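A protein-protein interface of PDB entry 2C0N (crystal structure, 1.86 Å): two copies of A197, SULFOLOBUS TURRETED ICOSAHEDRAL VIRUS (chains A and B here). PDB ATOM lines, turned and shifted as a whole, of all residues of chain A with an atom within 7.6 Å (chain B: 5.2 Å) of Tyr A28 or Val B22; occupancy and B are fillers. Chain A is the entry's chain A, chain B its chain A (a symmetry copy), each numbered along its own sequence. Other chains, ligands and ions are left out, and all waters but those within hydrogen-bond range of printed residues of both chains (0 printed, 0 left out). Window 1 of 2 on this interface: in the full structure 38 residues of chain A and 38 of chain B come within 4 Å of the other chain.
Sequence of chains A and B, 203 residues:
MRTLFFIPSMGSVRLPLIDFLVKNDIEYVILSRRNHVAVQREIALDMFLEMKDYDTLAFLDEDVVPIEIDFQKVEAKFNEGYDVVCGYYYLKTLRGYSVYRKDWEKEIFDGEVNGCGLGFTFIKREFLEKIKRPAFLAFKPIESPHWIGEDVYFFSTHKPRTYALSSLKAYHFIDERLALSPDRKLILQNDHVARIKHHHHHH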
ATOM      1  N   THR A   3      -7.634   1.281 -11.791  1.00  0.00           N
ATOM      2  CA  THR A   3      -6.354   1.737 -12.300  1.00  0.00           C
ATOM      3  C   THR A   3      -6.560   2.753 -13.404  1.00  0.00           C
ATOM      4  O   THR A   3      -7.366   2.530 -14.326  1.00  0.00           O
ATOM      5  CB  THR A   3      -5.572   0.538 -12.838  1.00  0.00           C
ATOM      6  OG1 THR A   3      -5.441  -0.424 -11.783  1.00  0.00           O
ATOM      7  CG2 THR A   3      -4.208   0.925 -13.339  1.00  0.00           C
ATOM      8  N   LEU A   4      -5.816   3.848 -13.302  1.00  0.00           N
ATOM      9  CA  LEU A   4      -5.757   4.863 -14.313  1.00  0.00           C
ATOM     10  C   LEU A   4      -4.369   4.828 -14.949  1.00  0.00           C
ATOM     11  O   LEU A   4      -3.336   5.053 -14.274  1.00  0.00           O
ATOM     12  CB  LEU A   4      -6.030   6.238 -13.722  1.00  0.00           C
ATOM     13  CG  LEU A   4      -6.223   7.388 -14.710  1.00  0.00           C
ATOM     14  CD1 LEU A   4      -7.261   7.033 -15.750  1.00  0.00           C
ATOM     15  CD2 LEU A   4      -6.638   8.607 -13.967  1.00  0.00           C
ATOM     16  N   PHE A   5      -4.359   4.524 -16.246  1.00  0.00           N
ATOM     17  CA  PHE A   5      -3.120   4.466 -17.015  1.00  0.00           C
ATOM     18  C   PHE A   5      -2.702   5.855 -17.514  1.00  0.00           C
ATOM     19  O   PHE A   5      -3.481   6.557 -18.105  1.00  0.00           O
ATOM     20  CB  PHE A   5      -3.262   3.527 -18.211  1.00  0.00           C
ATOM     21  CG  PHE A   5      -3.192   2.086 -17.844  1.00  0.00           C
ATOM     22  CD1 PHE A   5      -4.256   1.484 -17.185  1.00  0.00           C
ATOM     23  CD2 PHE A   5      -2.079   1.329 -18.128  1.00  0.00           C
ATOM     24  CE1 PHE A   5      -4.192   0.154 -16.822  1.00  0.00           C
ATOM     25  CE2 PHE A   5      -2.001   0.001 -17.769  1.00  0.00           C
ATOM     26  CZ  PHE A   5      -3.086  -0.586 -17.118  1.00  0.00           C
ATOM     27  N   PHE A   6      -1.448   6.211 -17.312  1.00  0.00           N
ATOM     28  CA  PHE A   6      -0.918   7.454 -17.846  1.00  0.00           C
ATOM     29  C   PHE A   6       0.158   7.065 -18.829  1.00  0.00           C
ATOM     30  O   PHE A   6       1.107   6.356 -18.480  1.00  0.00           O
ATOM     31  CB  PHE A   6      -0.365   8.334 -16.740  1.00  0.00           C
ATOM     32  CG  PHE A   6      -1.437   9.001 -15.906  1.00  0.00           C
ATOM     33  CD1 PHE A   6      -2.038   8.323 -14.879  1.00  0.00           C
ATOM     34  CD2 PHE A   6      -1.869  10.280 -16.206  1.00  0.00           C
ATOM     35  CE1 PHE A   6      -3.048   8.911 -14.131  1.00  0.00           C
ATOM     36  CE2 PHE A   6      -2.868  10.879 -15.475  1.00  0.00           C
ATOM     37  CZ  PHE A   6      -3.454  10.209 -14.447  1.00  0.00           C
ATOM     38  N   ILE A   7      -0.016   7.520 -20.065  1.00  0.00           N
ATOM     39  CA  ILE A   7       0.826   7.132 -21.170  1.00  0.00           C
ATOM     40  C   ILE A   7       1.557   8.373 -21.708  1.00  0.00           C
ATOM     41  O   ILE A   7       0.953   9.158 -22.417  1.00  0.00           O
ATOM     42  CB  ILE A   7      -0.027   6.459 -22.271  1.00  0.00           C
ATOM     43  CG1 ILE A   7      -0.723   5.200 -21.716  1.00  0.00           C
ATOM     44  CG2 ILE A   7       0.875   6.225 -23.536  1.00  0.00           C
ATOM     45  CD1 ILE A   7      -1.961   4.702 -22.529  1.00  0.00           C
ATOM     46  N   VAL A  13      -0.038   7.670 -30.894  1.00  0.00           N
ATOM     47  CA  VAL A  13      -0.038   6.343 -30.297  1.00  0.00           C
ATOM     48  C   VAL A  13      -0.035   5.272 -31.412  1.00  0.00           C
ATOM     49  O   VAL A  13      -0.886   5.296 -32.303  1.00  0.00           O
ATOM     50  CB  VAL A  13      -1.255   6.137 -29.409  1.00  0.00           C
ATOM     51  CG1 VAL A  13      -1.237   4.784 -28.744  1.00  0.00           C
ATOM     52  CG2 VAL A  13      -1.257   7.208 -28.298  1.00  0.00           C
ATOM     53  N   LEU A  17      -0.662  -0.413 -29.394  1.00  0.00           N
ATOM     54  CA  LEU A  17      -1.111   0.111 -28.095  1.00  0.00           C
ATOM     55  C   LEU A  17      -2.595   0.507 -28.101  1.00  0.00           C
ATOM     56  O   LEU A  17      -3.309   0.182 -27.172  1.00  0.00           O
ATOM     57  CB  LEU A  17      -0.188   1.234 -27.570  1.00  0.00           C
ATOM     58  CG  LEU A  17      -0.586   1.827 -26.210  1.00  0.00           C
ATOM     59  CD1 LEU A  17      -0.467   0.829 -25.192  1.00  0.00           C
ATOM     60  CD2 LEU A  17       0.294   2.984 -25.920  1.00  0.00           C
ATOM     61  N   ILE A  18      -3.094   1.105 -29.188  1.00  0.00           N
ATOM     62  CA  ILE A  18      -4.513   1.377 -29.328  1.00  0.00           C
ATOM     63  C   ILE A  18      -5.307   0.110 -29.160  1.00  0.00           C
ATOM     64  O   ILE A  18      -6.339   0.091 -28.455  1.00  0.00           O
ATOM     65  CB  ILE A  18      -4.815   2.035 -30.648  1.00  0.00           C
ATOM     66  CG1 ILE A  18      -4.104   3.369 -30.701  1.00  0.00           C
ATOM     67  CG2 ILE A  18      -6.338   2.285 -30.836  1.00  0.00           C
ATOM     68  CD1 ILE A  18      -4.247   4.013 -32.020  1.00  0.00           C
ATOM     69  N   LEU A  21      -5.472  -0.918 -25.592  1.00  0.00           N
ATOM     70  CA  LEU A  21      -6.389   0.005 -24.881  1.00  0.00           C
ATOM     71  C   LEU A  21      -7.868  -0.315 -25.092  1.00  0.00           C
ATOM     72  O   LEU A  21      -8.661  -0.320 -24.107  1.00  0.00           O
ATOM     73  CB  LEU A  21      -6.080   1.461 -25.213  1.00  0.00           C
ATOM     74  CG  LEU A  21      -4.704   1.969 -24.791  1.00  0.00           C
ATOM     75  CD1 LEU A  21      -4.551   3.402 -25.282  1.00  0.00           C
ATOM     76  CD2 LEU A  21      -4.534   1.907 -23.258  1.00  0.00           C
ATOM     77  N   VAL A  22      -8.240  -0.624 -26.341  1.00  0.00           N
ATOM     78  CA  VAL A  22      -9.617  -0.927 -26.698  1.00  0.00           C
ATOM     79  C   VAL A  22     -10.043  -2.296 -26.157  1.00  0.00           C
ATOM     80  O   VAL A  22     -11.082  -2.443 -25.497  1.00  0.00           O
ATOM     81  CB  VAL A  22      -9.797  -0.878 -28.252  1.00  0.00           C
ATOM     82  CG1 VAL A  22     -11.154  -1.410 -28.697  1.00  0.00           C
ATOM     83  CG2 VAL A  22      -9.611   0.520 -28.698  1.00  0.00           C
ATOM     84  N   ASP A  25     -10.498  -2.385 -22.312  1.00  0.00           N
ATOM     85  CA  ASP A  25     -11.384  -1.403 -21.674  1.00  0.00           C
ATOM     86  C   ASP A  25     -10.620  -0.494 -20.703  1.00  0.00           C
ATOM     87  O   ASP A  25     -11.114  -0.111 -19.673  1.00  0.00           O
ATOM     88  CB  ASP A  25     -12.515  -2.132 -20.973  1.00  0.00           C
ATOM     89  CG  ASP A  25     -13.699  -1.234 -20.635  1.00  0.00           C
ATOM     90  OD1 ASP A  25     -13.803  -0.119 -21.183  1.00  0.00           O
ATOM     91  OD2 ASP A  25     -14.544  -1.678 -19.820  1.00  0.00           O
ATOM     92  N   ILE A  26      -9.432  -0.078 -21.121  1.00  0.00           N
ATOM     93  CA  ILE A  26      -8.511   0.627 -20.237  1.00  0.00           C
ATOM     94  C   ILE A  26      -8.967   2.071 -20.080  1.00  0.00           C
ATOM     95  O   ILE A  26      -9.410   2.695 -21.061  1.00  0.00           O
ATOM     96  CB  ILE A  26      -7.121   0.643 -20.859  1.00  0.00           C
ATOM     97  CG1 ILE A  26      -6.590  -0.775 -21.005  1.00  0.00           C
ATOM     98  CG2 ILE A  26      -6.170   1.568 -20.079  1.00  0.00           C
ATOM     99  CD1 ILE A  26      -6.309  -1.517 -19.720  1.00  0.00           C
ATOM    100  N   GLU A  27      -8.871   2.585 -18.854  1.00  0.00           N
ATOM    101  CA  GLU A  27      -9.062   4.011 -18.577  1.00  0.00           C
ATOM    102  C   GLU A  27      -7.689   4.687 -18.532  1.00  0.00           C
ATOM    103  O   GLU A  27      -6.762   4.187 -17.886  1.00  0.00           O
ATOM    104  CB  GLU A  27      -9.791   4.216 -17.263  1.00  0.00           C
ATOM    105  CG  GLU A  27     -11.224   3.719 -17.323  1.00  0.00           C
ATOM    106  CD  GLU A  27     -11.941   4.010 -16.059  1.00  0.00           C
ATOM    107  OE1 GLU A  27     -11.853   3.189 -15.126  1.00  0.00           O
ATOM    108  OE2 GLU A  27     -12.576   5.066 -15.980  1.00  0.00           O
ATOM    109  N   TYR A  28      -7.547   5.797 -19.256  1.00  0.00           N
ATOM    110  CA  TYR A  28      -6.226   6.370 -19.450  1.00  0.00           C
ATOM    111  C   TYR A  28      -6.251   7.862 -19.659  1.00  0.00           C
ATOM    112  O   TYR A  28      -7.290   8.465 -19.970  1.00  0.00           O
ATOM    113  CB  TYR A  28      -5.544   5.709 -20.662  1.00  0.00           C
ATOM    114  CG  TYR A  28      -6.352   5.864 -21.955  1.00  0.00           C
ATOM    115  CD1 TYR A  28      -6.306   7.050 -22.666  1.00  0.00           C
ATOM    116  CD2 TYR A  28      -7.139   4.840 -22.452  1.00  0.00           C
ATOM    117  CE1 TYR A  28      -6.987   7.219 -23.847  1.00  0.00           C
ATOM    118  CE2 TYR A  28      -7.853   5.002 -23.656  1.00  0.00           C
ATOM    119  CZ  TYR A  28      -7.764   6.198 -24.338  1.00  0.00           C
ATOM    120  OH  TYR A  28      -8.461   6.401 -25.510  1.00  0.00           O
ATOM    121  N   VAL A  29      -5.058   8.431 -19.522  1.00  0.00           N
ATOM    122  CA  VAL A  29      -4.739   9.730 -19.996  1.00  0.00           C
ATOM    123  C   VAL A  29      -3.459   9.605 -20.825  1.00  0.00           C
ATOM    124  O   VAL A  29      -2.421   9.157 -20.333  1.00  0.00           O
ATOM    125  CB  VAL A  29      -4.496  10.709 -18.874  1.00  0.00           C
ATOM    126  CG1 VAL A  29      -4.109  12.080 -19.430  1.00  0.00           C
ATOM    127  CG2 VAL A  29      -5.744  10.848 -17.995  1.00  0.00           C
ATOM    128  N   ILE A  30      -3.558   9.938 -22.089  1.00  0.00           N
ATOM    129  CA  ILE A  30      -2.391   9.976 -22.939  1.00  0.00           C
ATOM    130  C   ILE A  30      -1.868  11.409 -22.888  1.00  0.00           C
ATOM    131  O   ILE A  30      -2.590  12.334 -23.193  1.00  0.00           O
ATOM    132  CB  ILE A  30      -2.701   9.627 -24.396  1.00  0.00           C
ATOM    133  CG1 ILE A  30      -3.426   8.294 -24.482  1.00  0.00           C
ATOM    134  CG2 ILE A  30      -1.395   9.485 -25.166  1.00  0.00           C
ATOM    135  CD1 ILE A  30      -4.031   8.026 -25.798  1.00  0.00           C
ATOM    136  N   LEU A  31      -0.625  11.582 -22.474  1.00  0.00           N
ATOM    137  CA  LEU A  31      -0.078  12.891 -22.211  1.00  0.00           C
ATOM    138  C   LEU A  31       0.584  13.386 -23.481  1.00  0.00           C
ATOM    139  O   LEU A  31       1.421  12.673 -24.067  1.00  0.00           O
ATOM    140  CB  LEU A  31       0.941  12.820 -21.070  1.00  0.00           C
ATOM    141  CG  LEU A  31       0.310  12.311 -19.758  1.00  0.00           C
ATOM    142  CD1 LEU A  31       1.288  11.575 -18.902  1.00  0.00           C
ATOM    143  CD2 LEU A  31      -0.273  13.438 -19.040  1.00  0.00           C
ATOM    144  N   MET A  47      -2.674  15.081 -11.719  1.00  0.00           N
ATOM    145  CA  MET A  47      -4.008  14.709 -12.158  1.00  0.00           C
ATOM    146  C   MET A  47      -4.521  13.494 -11.350  1.00  0.00           C
ATOM    147  O   MET A  47      -5.620  13.510 -10.826  1.00  0.00           O
ATOM    148  CB  MET A  47      -4.010  14.375 -13.641  1.00  0.00           C
ATOM    149  CG  MET A  47      -3.798  15.605 -14.576  1.00  0.00           C
ATOM    150  SD  MET A  47      -3.705  15.000 -16.423  1.00  0.00           S
ATOM    151  CE  MET A  47      -5.567  14.340 -16.548  1.00  0.00           C
ATOM    152  N   MET A  51      -7.998  12.649  -8.798  1.00  0.00           N
ATOM    153  CA  MET A  51      -9.014  11.725  -9.288  1.00  0.00           C
ATOM    154  C   MET A  51      -9.218  10.515  -8.333  1.00  0.00           C
ATOM    155  O   MET A  51      -8.785   9.398  -8.597  1.00  0.00           O
ATOM    156  CB  MET A  51      -8.678  11.338 -10.724  1.00  0.00           C
ATOM    157  CG  MET A  51      -8.754  12.550 -11.695  1.00  0.00           C
ATOM    158  SD  MET A  51      -7.766  12.305 -13.358  1.00  0.00           S
ATOM    159  CE  MET A  51      -9.028  11.159 -14.170  1.00  0.00           C
ATOM    160  N   TYR A  54      -9.685   6.536  -8.475  1.00  0.00           N
ATOM    161  CA  TYR A  54      -8.633   5.668  -8.974  1.00  0.00           C
ATOM    162  C   TYR A  54      -7.678   5.379  -7.844  1.00  0.00           C
ATOM    163  O   TYR A  54      -7.293   6.280  -7.125  1.00  0.00           O
ATOM    164  CB  TYR A  54      -7.956   6.296 -10.197  1.00  0.00           C
ATOM    165  CG  TYR A  54      -8.979   6.447 -11.297  1.00  0.00           C
ATOM    166  CD1 TYR A  54      -9.698   7.608 -11.428  1.00  0.00           C
ATOM    167  CD2 TYR A  54      -9.279   5.397 -12.160  1.00  0.00           C
ATOM    168  CE1 TYR A  54     -10.679   7.745 -12.411  1.00  0.00           C
ATOM    169  CE2 TYR A  54     -10.270   5.524 -13.140  1.00  0.00           C
ATOM    170  CZ  TYR A  54     -10.959   6.702 -13.266  1.00  0.00           C
ATOM    171  OH  TYR A  54     -11.972   6.850 -14.225  1.00  0.00           O
ATOM    172  N   ALA A  58      -1.008   3.704 -13.093  1.00  0.00           N
ATOM    173  CA  ALA A  58      -0.171   2.847 -13.926  1.00  0.00           C
ATOM    174  C   ALA A  58       0.502   3.721 -14.963  1.00  0.00           C
ATOM    175  O   ALA A  58      -0.196   4.403 -15.728  1.00  0.00           O
ATOM    176  CB  ALA A  58      -1.001   1.799 -14.600  1.00  0.00           C
ATOM    177  N   ARG A 195     -12.681  -0.961 -33.372  1.00  0.00           N
ATOM    178  CA  ARG A 195     -13.582  -0.731 -32.246  1.00  0.00           C
ATOM    179  C   ARG A 195     -14.980  -0.705 -32.885  1.00  0.00           C
ATOM    180  O   ARG A 195     -15.402   0.272 -33.506  1.00  0.00           O
ATOM    181  CB  ARG A 195     -13.171   0.556 -31.555  1.00  0.00           C
ATOM    182  CG  ARG A 195     -13.828   0.826 -30.220  1.00  0.00           C
ATOM    183  CD  ARG A 195     -14.944   1.782 -30.377  1.00  0.00           C
ATOM    184  NE  ARG A 195     -15.678   1.953 -29.132  1.00  0.00           N
ATOM    185  CZ  ARG A 195     -16.800   2.649 -29.012  1.00  0.00           C
ATOM    186  NH1 ARG A 195     -17.343   3.256 -30.058  1.00  0.00           N
ATOM    187  NH2 ARG A 195     -17.394   2.723 -27.832  1.00  0.00           N
ATOM    188  N   LEU B  17      -6.745  13.104 -33.221  1.00  0.00           N
ATOM    189  CA  LEU B  17      -7.708  12.150 -33.792  1.00  0.00           C
ATOM    190  C   LEU B  17      -8.228  11.144 -32.753  1.00  0.00           C
ATOM    191  O   LEU B  17      -9.416  10.891 -32.702  1.00  0.00           O
ATOM    192  CB  LEU B  17      -7.167  11.472 -35.071  1.00  0.00           C
ATOM    193  CG  LEU B  17      -8.122  10.468 -35.734  1.00  0.00           C
ATOM    194  CD1 LEU B  17      -9.285  11.148 -36.214  1.00  0.00           C
ATOM    195  CD2 LEU B  17      -7.408   9.795 -36.845  1.00  0.00           C
ATOM    196  N   ILE B  18      -7.371  10.656 -31.851  1.00  0.00           N
ATOM    197  CA  ILE B  18      -7.814   9.818 -30.751  1.00  0.00           C
ATOM    198  C   ILE B  18      -8.884  10.517 -29.959  1.00  0.00           C
ATOM    199  O   ILE B  18      -9.915   9.909 -29.601  1.00  0.00           O
ATOM    200  CB  ILE B  18      -6.660   9.418 -29.870  1.00  0.00           C
ATOM    201  CG1 ILE B  18      -5.686   8.596 -30.685  1.00  0.00           C
ATOM    202  CG2 ILE B  18      -7.125   8.564 -28.658  1.00  0.00           C
ATOM    203  CD1 ILE B  18      -4.464   8.280 -29.922  1.00  0.00           C
ATOM    204  N   ASP B  19      -8.669  11.802 -29.682  1.00  0.00           N
ATOM    205  CA  ASP B  19      -9.655  12.577 -28.905  1.00  0.00           C
ATOM    206  C   ASP B  19     -11.003  12.676 -29.596  1.00  0.00           C
ATOM    207  O   ASP B  19     -12.056  12.491 -28.957  1.00  0.00           O
ATOM    208  CB  ASP B  19      -9.101  13.963 -28.590  1.00  0.00           C
ATOM    209  CG  ASP B  19      -9.713  14.560 -27.356  1.00  0.00           C
ATOM    210  OD1 ASP B  19     -10.005  13.815 -26.374  1.00  0.00           O
ATOM    211  OD2 ASP B  19      -9.930  15.778 -27.388  1.00  0.00           O
ATOM    212  N   PHE B  20     -10.981  12.939 -30.899  1.00  0.00           N
ATOM    213  CA  PHE B  20     -12.193  12.952 -31.687  1.00  0.00           C
ATOM    214  C   PHE B  20     -12.898  11.587 -31.602  1.00  0.00           C
ATOM    215  O   PHE B  20     -14.127  11.521 -31.416  1.00  0.00           O
ATOM    216  CB  PHE B  20     -11.865  13.261 -33.160  1.00  0.00           C
ATOM    217  CG  PHE B  20     -12.973  12.922 -34.096  1.00  0.00           C
ATOM    218  CD1 PHE B  20     -14.070  13.756 -34.198  1.00  0.00           C
ATOM    219  CD2 PHE B  20     -12.959  11.759 -34.809  1.00  0.00           C
ATOM    220  CE1 PHE B  20     -15.114  13.459 -35.100  1.00  0.00           C
ATOM    221  CE2 PHE B  20     -13.964  11.475 -35.683  1.00  0.00           C
ATOM    222  CZ  PHE B  20     -15.045  12.306 -35.811  1.00  0.00           C
ATOM    223  N   LEU B  21     -12.130  10.508 -31.768  1.00  0.00           N
ATOM    224  CA  LEU B  21     -12.689   9.135 -31.718  1.00  0.00           C
ATOM    225  C   LEU B  21     -13.371   8.799 -30.394  1.00  0.00           C
ATOM    226  O   LEU B  21     -14.497   8.220 -30.390  1.00  0.00           O
ATOM    227  CB  LEU B  21     -11.639   8.094 -32.087  1.00  0.00           C
ATOM    228  CG  LEU B  21     -11.082   8.173 -33.505  1.00  0.00           C
ATOM    229  CD1 LEU B  21      -9.995   7.117 -33.654  1.00  0.00           C
ATOM    230  CD2 LEU B  21     -12.193   7.949 -34.553  1.00  0.00           C
ATOM    231  N   VAL B  22     -12.738   9.187 -29.279  1.00  0.00           N
ATOM    232  CA  VAL B  22     -13.254   8.914 -27.947  1.00  0.00           C
ATOM    233  C   VAL B  22     -14.479   9.781 -27.637  1.00  0.00           C
ATOM    234  O   VAL B  22     -15.537   9.290 -27.217  1.00  0.00           O
ATOM    235  CB  VAL B  22     -12.138   9.151 -26.876  1.00  0.00           C
ATOM    236  CG1 VAL B  22     -12.680   9.104 -25.452  1.00  0.00           C
ATOM    237  CG2 VAL B  22     -11.086   8.129 -27.068  1.00  0.00           C
ATOM    238  N   LYS B  23     -14.319  11.078 -27.853  1.00  0.00           N
ATOM    239  CA  LYS B  23     -15.338  12.041 -27.477  1.00  0.00           C
ATOM    240  C   LYS B  23     -16.642  11.810 -28.222  1.00  0.00           C
ATOM    241  O   LYS B  23     -17.718  12.063 -27.666  1.00  0.00           O
ATOM    242  CB  LYS B  23     -14.850  13.463 -27.717  1.00  0.00           C
ATOM    243  CG  LYS B  23     -14.015  13.982 -26.588  1.00  0.00           C
ATOM    244  CD  LYS B  23     -13.314  15.278 -26.929  1.00  0.00           C
ATOM    245  CE  LYS B  23     -12.847  15.977 -25.658  1.00  0.00           C
ATOM    246  NZ  LYS B  23     -11.575  16.701 -25.816  1.00  0.00           N
ATOM    247  N   ASN B  24     -16.553  11.296 -29.447  1.00  0.00           N
ATOM    248  CA  ASN B  24     -17.717  11.110 -30.294  1.00  0.00           C
ATOM    249  C   ASN B  24     -18.200   9.665 -30.434  1.00  0.00           C
ATOM    250  O   ASN B  24     -19.077   9.376 -31.239  1.00  0.00           O
ATOM    251  CB  ASN B  24     -17.445  11.720 -31.661  1.00  0.00           C
ATOM    252  CG  ASN B  24     -17.249  13.204 -31.574  1.00  0.00           C
ATOM    253  OD1 ASN B  24     -18.222  13.950 -31.511  1.00  0.00           O
ATOM    254  ND2 ASN B  24     -15.988  13.653 -31.556  1.00  0.00           N
ATOM    255  N   ASP B  25     -17.652   8.766 -29.612  1.00  0.00           N
ATOM    256  CA  ASP B  25     -18.115   7.374 -29.556  1.00  0.00           C
ATOM    257  C   ASP B  25     -18.084   6.707 -30.936  1.00  0.00           C
ATOM    258  O   ASP B  25     -18.927   5.917 -31.277  1.00  0.00           O
ATOM    259  CB  ASP B  25     -19.508   7.336 -28.955  1.00  0.00           C
ATOM    260  CG  ASP B  25     -19.922   5.951 -28.471  1.00  0.00           C
ATOM    261  OD1 ASP B  25     -19.056   5.068 -28.315  1.00  0.00           O
ATOM    262  OD2 ASP B  25     -21.139   5.769 -28.223  1.00  0.00           O
ATOM    263  N   VAL B 193      -5.165  13.600 -23.837  1.00  0.00           N
ATOM    264  CA  VAL B 193      -6.371  12.912 -24.280  1.00  0.00           C
ATOM    265  C   VAL B 193      -6.752  11.893 -23.233  1.00  0.00           C
ATOM    266  O   VAL B 193      -5.951  11.044 -22.897  1.00  0.00           O
ATOM    267  CB  VAL B 193      -6.157  12.233 -25.620  1.00  0.00           C
ATOM    268  CG1 VAL B 193      -7.424  11.522 -26.065  1.00  0.00           C
ATOM    269  CG2 VAL B 193      -5.726  13.301 -26.640  1.00  0.00           C
ATOM    270  N   ALA B 194      -7.983  11.978 -22.753  1.00  0.00           N
ATOM    271  CA  ALA B 194      -8.455  11.165 -21.647  1.00  0.00           C
ATOM    272  C   ALA B 194      -9.644  10.323 -22.065  1.00  0.00           C
ATOM    273  O   ALA B 194     -10.500  10.744 -22.831  1.00  0.00           O
ATOM    274  CB  ALA B 194      -8.850  12.018 -20.464  1.00  0.00           C
ATOM    275  N   ARG B 195      -9.653   9.112 -21.550  1.00  0.00           N
ATOM    276  CA  ARG B 195     -10.830   8.250 -21.605  1.00  0.00           C
ATOM    277  C   ARG B 195     -10.994   7.748 -20.162  1.00  0.00           C
ATOM    278  O   ARG B 195     -10.285   6.859 -19.688  1.00  0.00           O
ATOM    279  CB  ARG B 195     -10.584   7.162 -22.635  1.00  0.00           C
ATOM    280  CG  ARG B 195     -11.787   6.327 -23.011  1.00  0.00           C
ATOM    281  CD  ARG B 195     -11.766   5.037 -22.290  1.00  0.00           C
ATOM    282  NE  ARG B 195     -12.981   4.273 -22.530  1.00  0.00           N
ATOM    283  CZ  ARG B 195     -13.291   3.142 -21.912  1.00  0.00           C
ATOM    284  NH1 ARG B 195     -12.482   2.616 -21.003  1.00  0.00           N
ATOM    285  NH2 ARG B 195     -14.434   2.540 -22.198  1.00  0.00           N
ATOM    286  N   ILE B 196     -11.901   8.394 -19.453  1.00  0.00           N
ATOM    287  CA  ILE B 196     -12.055   8.163 -18.023  1.00  0.00           C
ATOM    288  C   ILE B 196     -13.537   8.035 -17.796  1.00  0.00           C
ATOM    289  O   ILE B 196     -14.294   8.912 -18.192  1.00  0.00           O
ATOM    290  CB  ILE B 196     -11.458   9.305 -17.138  1.00  0.00           C
ATOM    291  CG1 ILE B 196     -11.970  10.678 -17.582  1.00  0.00           C
ATOM    292  CG2 ILE B 196      -9.932   9.262 -17.135  1.00  0.00           C
ATOM    293  CD1 ILE B 196     -12.995  11.272 -16.690  1.00  0.00           C
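Hydrophobic or aromatic side chains of chain B that line the printed part of chain A: Ile B18, Val B22, Ala B194 and Ile B196.
Hydrophobic or aromatic side chains of chain A that line the printed part of chain B: Leu A4, Val A13, Tyr A28, Ile A30, Met A51 and Tyr A54.
Among the printed residues, 15 pairs touch across the chains.
Leu A4 touches Ile B196 (CD1 to CG2, 3.7 Å).
CG2 of Val A13 touches CD1 of Ile B18, 3.8 Å away.
O of Arg B195 touches CA of Glu A27, at 3.3 Å.
OE2 of Glu A27 touches C of Ile B196, at 3.6 Å.
Val B22 touches Tyr A28 (CG2 to OH, 3.5 Å).
O of Tyr A28 touches CA of Ala B194 (3.4 Å).
Tyr A28 touches Ile B196.
CA of Val A29 touches O of Val B193, 3.4 Å away.
Ile B196 touches Met A51.
OH of Tyr A54 touches CB of Ile B196 (3.8 Å).
O of Ile A26 sits at hydrogen-bond distance from NH1 of Arg B195 (3.1 Å).
The side-chain carboxylate of Asp B25 is in salt-bridge range of the guanidinium group of Arg A195 (2.9 Å).
The backbone NH (N) of Arg B195 sits at hydrogen-bond distance from the backbone carbonyl oxygen (O) of Tyr A28 (2.9 Å).
OD1 of Asp A25 lies within salt-bridge range of NH2 of Arg B195, at 2.9 Å.
O of Val B193 is in hydrogen-bond range of N of Ile A30 (2.8 Å).
Asp A25 touches Arg B195, and with the chains exchanged Arg A195 touches Asp B25.
Of the 15 pairs that touch across the chains among the printed residues, 2 have their exchanged pair printed and touching as well.
Ile A7 touches none of the printed residues of chain B.
Of the printed residues of chain B, Ile A26 touches Arg B195.
Of the printed residues of chain B, Tyr A28 touches Val B22, Ala B194, Arg B195 and Ile B196.
Printed residues of chain B within 4 Å of Val A29: Val B193 (3.4 Å).
Printed residues of chain B within 4 Å of Arg A195: Asp B25 (2.9 Å).
Val B22 touches just one residue of chain A: Tyr A28.
Printed residues of chain A within 4 Å of Ile B196: Leu A4, Glu A27, Tyr A28, Met A51 and Tyr A54.
The nearest printed residue of chain B that does not touch Tyr A28 is Val B193 (4.02 Å).
The backbone carbonyl oxygen (O) of Leu A21 sits at hydrogen-bond distance from the backbone NH (N) of Ile A26 (3.1 Å).
N of Ala A58 sits at hydrogen-bond distance from O of Leu A4 (2.9 Å).
The backbone carbonyl oxygen (O) of Val A29 sits at hydrogen-bond distance from the backbone NH (N) of Ile A7, 2.9 Å away.
The side-chain hydroxyl (OH) of Tyr A54 lies within hydrogen-bond range of the side-chain carboxylate (OE2) of Glu A27 (2.6 Å).
O of Phe A5 is in hydrogen-bond range of N of Val A29 (2.8 Å).
The backbone carbonyl oxygen (O) of Glu A27 sits at hydrogen-bond distance from the backbone NH (N) of Phe A5 (2.9 Å).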
